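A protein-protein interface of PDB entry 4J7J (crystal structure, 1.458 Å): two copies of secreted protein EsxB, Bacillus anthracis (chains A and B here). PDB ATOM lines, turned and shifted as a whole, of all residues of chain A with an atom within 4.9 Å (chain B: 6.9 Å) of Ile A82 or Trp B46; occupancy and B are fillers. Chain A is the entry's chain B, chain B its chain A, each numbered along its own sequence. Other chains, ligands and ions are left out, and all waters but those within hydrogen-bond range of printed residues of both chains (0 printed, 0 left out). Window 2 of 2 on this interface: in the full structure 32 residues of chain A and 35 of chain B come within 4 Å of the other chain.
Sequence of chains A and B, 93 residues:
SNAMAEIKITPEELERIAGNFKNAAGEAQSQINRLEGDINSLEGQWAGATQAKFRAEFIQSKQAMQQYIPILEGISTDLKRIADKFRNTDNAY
O of Gln B45 lies within hydrogen-bond range of N of Ile A9 (3.3 Å). The side-chain amino group of Lys B53 is in salt-bridge range of the side-chain carboxylate of Asp A78, 3.1 Å away.
O of Leu B42 sits close to NE1 of Trp B46, 3.4 Å away. The side-chain amide oxygen (OE1) of Gln B51 sits close to the backbone carbonyl oxygen (O) of Leu B42 (3.4 Å). OE1 of Gln B51 sits at hydrogen-bond distance from NE1 of Trp B46 (2.9 Å). The guanidinium group (NH2) of Arg A81 is in salt-bridge range of the side-chain carboxylate (OD1) of Asp A78 (3.1 Å).
Ile A7 touches Gln B45 (CG2 to O, 3.9 Å). Leu B42 touches Ile A9 (CD2 to CD1, 3.6 Å). Leu B42 touches Leu A14. Leu A14 touches Trp B46 (CD2 to CZ3, 3.6 Å). Asp A78 touches Phe B54 (CB to CZ, 3.7 Å). CD2 of Leu A79 touches CH2 of Trp B46 (3.9 Å). Phe B54 touches Leu A79. Trp B46 touches Ile A82. CD1 of Ile A82 touches CE2 of Phe B54, 3.4 Å away.
Of the printed residues of chain B, Asp A78 touches Lys B53 (3.1 Å) and Phe B54 (3.7 Å). Of the printed residues of chain B, Ile A9 touches Leu B42 and Gln B45. Printed residues of chain B within 4 Å of Leu A79: Trp B46 (3.9 Å) and Phe B54 (3.6 Å). Printed residues of chain B within 4 Å of Ile A7: Gln B45 (3.9 Å). Glu B43 touches none of the printed residues of chain A. Ala B52 touches none of the printed residues of chain A. The nearest residue of chain B that does not touch Ile A82 is Thr B50 (4.2 Å).
Of the 13 printed residues of chain A, 6 touch a printed residue of chain B. Printed residues of chain A that touch a printed residue of chain B: Ile A7, Ile A9, Leu A14, Asp A78, Leu A79 and Ile A82. Along chain A the printed residues that touch a printed residue of chain B span positions 7 to 82.
No position is printed for both chains. Of the 11 pairs that touch across the chains among the printed residues, none has its exchanged pair printed and touching as well.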
ATOM      1  N   ILE A   7      26.470 -37.326  23.622  1.00  0.00           N
ATOM      2  CA  ILE A   7      26.279 -35.882  23.594  1.00  0.00           C
ATOM      3  C   ILE A   7      25.185 -35.528  22.586  1.00  0.00           C
ATOM      4  O   ILE A   7      25.218 -35.987  21.445  1.00  0.00           O
ATOM      5  CB  ILE A   7      27.587 -35.182  23.175  1.00  0.00           C
ATOM      6  CG1 ILE A   7      28.769 -35.672  24.020  1.00  0.00           C
ATOM      7  CG2 ILE A   7      27.442 -33.686  23.250  1.00  0.00           C
ATOM      8  CD1 ILE A   7      28.542 -35.621  25.523  1.00  0.00           C
ATOM      9  N   ILE A   9      23.987 -32.139  22.289  1.00  0.00           N
ATOM     10  CA  ILE A   9      24.245 -30.779  21.849  1.00  0.00           C
ATOM     11  C   ILE A   9      25.197 -30.739  20.649  1.00  0.00           C
ATOM     12  O   ILE A   9      26.147 -31.511  20.572  1.00  0.00           O
ATOM     13  CB  ILE A   9      24.778 -29.905  23.019  1.00  0.00           C
ATOM     14  CG1 ILE A   9      24.553 -28.424  22.725  1.00  0.00           C
ATOM     15  CG2 ILE A   9      26.232 -30.229  23.361  1.00  0.00           C
ATOM     16  CD1 ILE A   9      23.208 -27.954  23.221  1.00  0.00           C
ATOM     17  N   LEU A  14      26.234 -24.782  20.706  1.00  0.00           N
ATOM     18  CA  LEU A  14      27.138 -24.279  21.736  1.00  0.00           C
ATOM     19  C   LEU A  14      27.658 -22.911  21.323  1.00  0.00           C
ATOM     20  O   LEU A  14      27.771 -22.001  22.147  1.00  0.00           O
ATOM     21  CB  LEU A  14      28.294 -25.250  21.969  1.00  0.00           C
ATOM     22  CG  LEU A  14      27.895 -26.548  22.671  1.00  0.00           C
ATOM     23  CD1 LEU A  14      29.052 -27.523  22.681  1.00  0.00           C
ATOM     24  CD2 LEU A  14      27.449 -26.240  24.096  1.00  0.00           C
ATOM     25  N   ASP A  78      34.601 -20.784  27.047  1.00  0.00           N
ATOM     26  CA  ASP A  78      34.581 -22.200  27.416  1.00  0.00           C
ATOM     27  C   ASP A  78      33.616 -22.972  26.518  1.00  0.00           C
ATOM     28  O   ASP A  78      33.895 -24.104  26.111  1.00  0.00           O
ATOM     29  CB  ASP A  78      34.201 -22.386  28.891  1.00  0.00           C
ATOM     30  CG  ASP A  78      35.298 -21.937  29.852  1.00  0.00           C
ATOM     31  OD1 ASP A  78      36.453 -21.752  29.414  1.00  0.00           O
ATOM     32  OD2 ASP A  78      34.998 -21.782  31.056  1.00  0.00           O
ATOM     33  N   LEU A  79      32.482 -22.362  26.202  1.00  0.00           N
ATOM     34  CA  LEU A  79      31.524 -22.948  25.264  1.00  0.00           C
ATOM     35  C   LEU A  79      32.136 -23.131  23.865  1.00  0.00           C
ATOM     36  O   LEU A  79      31.983 -24.186  23.251  1.00  0.00           O
ATOM     37  CB  LEU A  79      30.253 -22.094  25.194  1.00  0.00           C
ATOM     38  CG  LEU A  79      29.365 -22.146  26.441  1.00  0.00           C
ATOM     39  CD1 LEU A  79      28.322 -21.058  26.357  1.00  0.00           C
ATOM     40  CD2 LEU A  79      28.699 -23.500  26.577  1.00  0.00           C
ATOM     41  N   LYS A  80      32.840 -22.117  23.371  1.00  0.00           N
ATOM     42  CA  LYS A  80      33.483 -22.213  22.064  1.00  0.00           C
ATOM     43  C   LYS A  80      34.583 -23.265  22.062  1.00  0.00           C
ATOM     44  O   LYS A  80      34.778 -23.970  21.072  1.00  0.00           O
ATOM     45  CB  LYS A  80      34.063 -20.865  21.640  1.00  0.00           C
ATOM     46  CG  LYS A  80      33.017 -19.823  21.315  1.00  0.00           C
ATOM     47  CD  LYS A  80      33.661 -18.507  20.902  1.00  0.00           C
ATOM     48  CE  LYS A  80      34.341 -18.622  19.548  1.00  0.00           C
ATOM     49  NZ  LYS A  80      33.367 -18.809  18.439  1.00  0.00           N
ATOM     50  N   ARG A  81      35.310 -23.368  23.170  1.00  0.00           N
ATOM     51  CA  ARG A  81      36.395 -24.338  23.254  1.00  0.00           C
ATOM     52  C   ARG A  81      35.828 -25.748  23.178  1.00  0.00           C
ATOM     53  O   ARG A  81      36.414 -26.623  22.544  1.00  0.00           O
ATOM     54  CB  ARG A  81      37.217 -24.144  24.535  1.00  0.00           C
ATOM     55  CG  ARG A  81      38.503 -24.963  24.541  1.00  0.00           C
ATOM     56  CD  ARG A  81      39.446 -24.585  25.679  1.00  0.00           C
ATOM     57  NE  ARG A  81      39.950 -23.218  25.566  1.00  0.00           N
ATOM     58  CZ  ARG A  81      39.493 -22.202  26.289  1.00  0.00           C
ATOM     59  NH1 ARG A  81      39.998 -20.982  26.136  1.00  0.00           N
ATOM     60  NH2 ARG A  81      38.527 -22.409  27.172  1.00  0.00           N
ATOM     61  N   ILE A  82      34.672 -25.964  23.792  1.00  0.00           N
ATOM     62  CA  ILE A  82      34.026 -27.273  23.728  1.00  0.00           C
ATOM     63  C   ILE A  82      33.431 -27.550  22.348  1.00  0.00           C
ATOM     64  O   ILE A  82      33.572 -28.653  21.826  1.00  0.00           O
ATOM     65  CB  ILE A  82      32.951 -27.415  24.818  1.00  0.00           C
ATOM     66  CG1 ILE A  82      33.615 -27.517  26.187  1.00  0.00           C
ATOM     67  CG2 ILE A  82      32.078 -28.631  24.571  1.00  0.00           C
ATOM     68  CD1 ILE A  82      32.661 -27.289  27.335  1.00  0.00           C
ATOM     69  N   ALA A  83      32.776 -26.557  21.755  1.00  0.00           N
ATOM     70  CA  ALA A  83      32.250 -26.704  20.395  1.00  0.00           C
ATOM     71  C   ALA A  83      33.347 -27.108  19.404  1.00  0.00           C
ATOM     72  O   ALA A  83      33.149 -27.988  18.565  1.00  0.00           O
ATOM     73  CB  ALA A  83      31.567 -25.419  19.944  1.00  0.00           C
ATOM     74  N   ASP A  84      34.506 -26.468  19.516  1.00  0.00           N
ATOM     75  CA  ASP A  84      35.650 -26.761  18.659  1.00  0.00           C
ATOM     76  C   ASP A  84      36.147 -28.188  18.857  1.00  0.00           C
ATOM     77  O   ASP A  84      36.509 -28.873  17.898  1.00  0.00           O
ATOM     78  CB  ASP A  84      36.784 -25.773  18.936  1.00  0.00           C
ATOM     79  CG  ASP A  84      38.010 -26.042  18.083  1.00  0.00           C
ATOM     80  OD1 ASP A  84      37.979 -25.704  16.880  1.00  0.00           O
ATOM     81  OD2 ASP A  84      39.002 -26.590  18.610  1.00  0.00           O
ATOM     82  N   LYS A  85      36.169 -28.628  20.111  1.00  0.00           N
ATOM     83  CA  LYS A  85      36.615 -29.978  20.435  1.00  0.00           C
ATOM     84  C   LYS A  85      35.635 -31.015  19.900  1.00  0.00           C
ATOM     85  O   LYS A  85      36.048 -32.043  19.358  1.00  0.00           O
ATOM     86  CB  LYS A  85      36.778 -30.130  21.950  1.00  0.00           C
ATOM     87  CG  LYS A  85      37.032 -31.557  22.403  1.00  0.00           C
ATOM     88  CD  LYS A  85      37.072 -31.682  23.918  1.00  0.00           C
ATOM     89  CE  LYS A  85      36.630 -33.076  24.346  1.00  0.00           C
ATOM     90  NZ  LYS A  85      36.931 -33.369  25.777  1.00  0.00           N
ATOM     91  N   PHE A  86      34.341 -30.746  20.057  1.00  0.00           N
ATOM     92  CA  PHE A  86      33.302 -31.637  19.546  1.00  0.00           C
ATOM     93  C   PHE A  86      33.350 -31.727  18.026  1.00  0.00           C
ATOM     94  O   PHE A  86      33.204 -32.813  17.457  1.00  0.00           O
ATOM     95  CB  PHE A  86      31.911 -31.149  19.966  1.00  0.00           C
ATOM     96  CG  PHE A  86      31.564 -31.417  21.407  1.00  0.00           C
ATOM     97  CD1 PHE A  86      32.441 -32.087  22.250  1.00  0.00           C
ATOM     98  CD2 PHE A  86      30.343 -30.998  21.918  1.00  0.00           C
ATOM     99  CE1 PHE A  86      32.106 -32.332  23.577  1.00  0.00           C
ATOM    100  CE2 PHE A  86      30.004 -31.239  23.241  1.00  0.00           C
ATOM    101  CZ  PHE A  86      30.885 -31.906  24.071  1.00  0.00           C
ATOM    102  N   ARG A  87      33.558 -30.592  17.364  1.00  0.00           N
ATOM    103  CA  ARG A  87      33.502 -30.541  15.905  1.00  0.00           C
ATOM    104  C   ARG A  87      34.691 -31.233  15.249  1.00  0.00           C
ATOM    105  O   ARG A  87      34.519 -32.020  14.316  1.00  0.00           O
ATOM    106  CB  ARG A  87      33.388 -29.094  15.407  1.00  0.00           C
ATOM    107  CG  ARG A  87      33.380 -28.958  13.893  1.00  0.00           C
ATOM    108  CD  ARG A  87      33.324 -27.505  13.444  1.00  0.00           C
ATOM    109  NE  ARG A  87      31.980 -26.940  13.540  1.00  0.00           N
ATOM    110  CZ  ARG A  87      31.623 -25.978  14.384  1.00  0.00           C
ATOM    111  NH1 ARG A  87      32.510 -25.454  15.220  1.00  0.00           N
ATOM    112  NH2 ARG A  87      30.375 -25.532  14.389  1.00  0.00           N
ATOM    113  N   ILE B  39      21.671 -21.576  30.106  1.00  0.00           N
ATOM    114  CA  ILE B  39      22.354 -22.580  30.917  1.00  0.00           C
ATOM    115  C   ILE B  39      21.414 -23.749  31.219  1.00  0.00           C
ATOM    116  O   ILE B  39      21.804 -24.909  31.107  1.00  0.00           O
ATOM    117  CB  ILE B  39      22.896 -21.960  32.227  1.00  0.00           C
ATOM    118  CG1 ILE B  39      23.976 -20.918  31.912  1.00  0.00           C
ATOM    119  CG2 ILE B  39      23.426 -23.041  33.167  1.00  0.00           C
ATOM    120  CD1 ILE B  39      25.190 -21.464  31.179  1.00  0.00           C
ATOM    121  N   LEU B  42      20.999 -26.449  28.557  1.00  0.00           N
ATOM    122  CA  LEU B  42      22.104 -27.381  28.343  1.00  0.00           C
ATOM    123  C   LEU B  42      21.978 -28.623  29.227  1.00  0.00           C
ATOM    124  O   LEU B  42      22.680 -29.614  29.026  1.00  0.00           O
ATOM    125  CB  LEU B  42      23.447 -26.688  28.580  1.00  0.00           C
ATOM    126  CG  LEU B  42      23.821 -25.607  27.556  1.00  0.00           C
ATOM    127  CD1 LEU B  42      24.993 -24.776  28.051  1.00  0.00           C
ATOM    128  CD2 LEU B  42      24.140 -26.224  26.211  1.00  0.00           C
ATOM    129  N   GLU B  43      21.077 -28.563  30.203  1.00  0.00           N
ATOM    130  CA  GLU B  43      20.798 -29.709  31.065  1.00  0.00           C
ATOM    131  C   GLU B  43      20.320 -30.915  30.266  1.00  0.00           C
ATOM    132  O   GLU B  43      19.389 -30.811  29.461  1.00  0.00           O
ATOM    133  CB  GLU B  43      19.734 -29.344  32.102  1.00  0.00           C
ATOM    134  CG  GLU B  43      20.248 -28.546  33.297  1.00  0.00           C
ATOM    135  CD  GLU B  43      20.358 -29.396  34.549  1.00  0.00           C
ATOM    136  OE1 GLU B  43      20.567 -30.622  34.419  1.00  0.00           O
ATOM    137  OE2 GLU B  43      20.227 -28.840  35.662  1.00  0.00           O
ATOM    138  N   GLY B  44      20.971 -32.056  30.484  1.00  0.00           N
ATOM    139  CA  GLY B  44      20.582 -33.313  29.861  1.00  0.00           C
ATOM    140  C   GLY B  44      21.052 -33.443  28.423  1.00  0.00           C
ATOM    141  O   GLY B  44      20.703 -34.399  27.720  1.00  0.00           O
ATOM    142  N   GLN B  45      21.856 -32.474  27.994  1.00  0.00           N
ATOM    143  CA  GLN B  45      22.330 -32.391  26.617  1.00  0.00           C
ATOM    144  C   GLN B  45      23.795 -32.810  26.500  1.00  0.00           C
ATOM    145  O   GLN B  45      24.306 -33.033  25.398  1.00  0.00           O
ATOM    146  CB  GLN B  45      22.148 -30.965  26.103  1.00  0.00           C
ATOM    147  CG  GLN B  45      20.694 -30.545  25.968  1.00  0.00           C
ATOM    148  CD  GLN B  45      20.049 -31.143  24.737  1.00  0.00           C
ATOM    149  OE1 GLN B  45      20.255 -30.665  23.620  1.00  0.00           O
ATOM    150  NE2 GLN B  45      19.278 -32.204  24.930  1.00  0.00           N
ATOM    151  N   TRP B  46      24.463 -32.891  27.648  1.00  0.00           N
ATOM    152  CA  TRP B  46      25.839 -33.371  27.748  1.00  0.00           C
ATOM    153  C   TRP B  46      26.090 -33.898  29.161  1.00  0.00           C
ATOM    154  O   TRP B  46      25.165 -33.967  29.972  1.00  0.00           O
ATOM    155  CB  TRP B  46      26.853 -32.278  27.374  1.00  0.00           C
ATOM    156  CG  TRP B  46      26.703 -30.972  28.118  1.00  0.00           C
ATOM    157  CD1 TRP B  46      25.891 -30.717  29.190  1.00  0.00           C
ATOM    158  CD2 TRP B  46      27.390 -29.742  27.840  1.00  0.00           C
ATOM    159  NE1 TRP B  46      26.030 -29.409  29.590  1.00  0.00           N
ATOM    160  CE2 TRP B  46      26.947 -28.790  28.777  1.00  0.00           C
ATOM    161  CE3 TRP B  46      28.337 -29.356  26.881  1.00  0.00           C
ATOM    162  CZ2 TRP B  46      27.416 -27.471  28.789  1.00  0.00           C
ATOM    163  CZ3 TRP B  46      28.808 -28.052  26.898  1.00  0.00           C
ATOM    164  CH2 TRP B  46      28.342 -27.122  27.841  1.00  0.00           C
ATOM    165  N   ALA B  47      27.337 -34.261  29.455  1.00  0.00           N
ATOM    166  CA  ALA B  47      27.667 -34.893  30.735  1.00  0.00           C
ATOM    167  C   ALA B  47      27.383 -33.998  31.941  1.00  0.00           C
ATOM    168  O   ALA B  47      27.511 -32.775  31.861  1.00  0.00           O
ATOM    169  CB  ALA B  47      29.118 -35.346  30.740  1.00  0.00           C
ATOM    170  N   GLY B  48      27.000 -34.619  33.056  1.00  0.00           N
ATOM    171  CA  GLY B  48      26.628 -33.901  34.263  1.00  0.00           C
ATOM    172  C   GLY B  48      27.746 -33.050  34.831  1.00  0.00           C
ATOM    173  O   GLY B  48      27.512 -31.953  35.341  1.00  0.00           O
ATOM    174  N   ALA B  49      28.971 -33.556  34.734  1.00  0.00           N
ATOM    175  CA  ALA B  49      30.137 -32.833  35.227  1.00  0.00           C
ATOM    176  C   ALA B  49      30.365 -31.562  34.415  1.00  0.00           C
ATOM    177  O   ALA B  49      30.841 -30.551  34.938  1.00  0.00           O
ATOM    178  CB  ALA B  49      31.363 -33.725  35.183  1.00  0.00           C
ATOM    179  N   THR B  50      30.028 -31.625  33.131  1.00  0.00           N
ATOM    180  CA  THR B  50      30.151 -30.479  32.252  1.00  0.00           C
ATOM    181  C   THR B  50      29.083 -29.451  32.614  1.00  0.00           C
ATOM    182  O   THR B  50      29.371 -28.254  32.750  1.00  0.00           O
ATOM    183  CB  THR B  50      30.012 -30.884  30.777  1.00  0.00           C
ATOM    184  OG1 THR B  50      30.951 -31.925  30.479  1.00  0.00           O
ATOM    185  CG2 THR B  50      30.272 -29.690  29.868  1.00  0.00           C
ATOM    186  N   GLN B  51      27.847 -29.917  32.784  1.00  0.00           N
ATOM    187  CA  GLN B  51      26.752 -29.029  33.180  1.00  0.00           C
ATOM    188  C   GLN B  51      27.023 -28.377  34.531  1.00  0.00           C
ATOM    189  O   GLN B  51      26.779 -27.179  34.707  1.00  0.00           O
ATOM    190  CB  GLN B  51      25.417 -29.780  33.216  1.00  0.00           C
ATOM    191  CG  GLN B  51      24.225 -28.924  33.630  1.00  0.00           C
ATOM    192  CD  GLN B  51      23.868 -27.864  32.599  1.00  0.00           C
ATOM    193  OE1 GLN B  51      24.299 -27.930  31.448  1.00  0.00           O
ATOM    194  NE2 GLN B  51      23.069 -26.887  33.010  1.00  0.00           N
ATOM    195  N   ALA B  52      27.531 -29.159  35.481  1.00  0.00           N
ATOM    196  CA  ALA B  52      27.858 -28.637  36.805  1.00  0.00           C
ATOM    197  C   ALA B  52      28.887 -27.514  36.720  1.00  0.00           C
ATOM    198  O   ALA B  52      28.768 -26.500  37.412  1.00  0.00           O
ATOM    199  CB  ALA B  52      28.358 -29.756  37.716  1.00  0.00           C
ATOM    200  N   LYS B  53      29.884 -27.686  35.854  1.00  0.00           N
ATOM    201  CA  LYS B  53      30.923 -26.673  35.690  1.00  0.00           C
ATOM    202  C   LYS B  53      30.339 -25.344  35.229  1.00  0.00           C
ATOM    203  O   LYS B  53      30.615 -24.292  35.809  1.00  0.00           O
ATOM    204  CB  LYS B  53      31.982 -27.137  34.692  1.00  0.00           C
ATOM    205  CG  LYS B  53      33.281 -26.359  34.809  1.00  0.00           C
ATOM    206  CD  LYS B  53      34.066 -26.374  33.512  1.00  0.00           C
ATOM    207  CE  LYS B  53      35.265 -25.443  33.599  1.00  0.00           C
ATOM    208  NZ  LYS B  53      35.313 -24.493  32.452  1.00  0.00           N
ATOM    209  N   PHE B  54      29.531 -25.395  34.178  1.00  0.00           N
ATOM    210  CA  PHE B  54      28.923 -24.192  33.636  1.00  0.00           C
ATOM    211  C   PHE B  54      27.897 -23.586  34.579  1.00  0.00           C
ATOM    212  O   PHE B  54      27.743 -22.368  34.631  1.00  0.00           O
ATOM    213  CB  PHE B  54      28.313 -24.473  32.270  1.00  0.00           C
ATOM    214  CG  PHE B  54      29.324 -24.517  31.179  1.00  0.00           C
ATOM    215  CD1 PHE B  54      29.727 -23.348  30.551  1.00  0.00           C
ATOM    216  CD2 PHE B  54      29.892 -25.715  30.792  1.00  0.00           C
ATOM    217  CE1 PHE B  54      30.676 -23.380  29.550  1.00  0.00           C
ATOM    218  CE2 PHE B  54      30.839 -25.754  29.788  1.00  0.00           C
ATOM    219  CZ  PHE B  54      31.231 -24.579  29.167  1.00  0.00           C
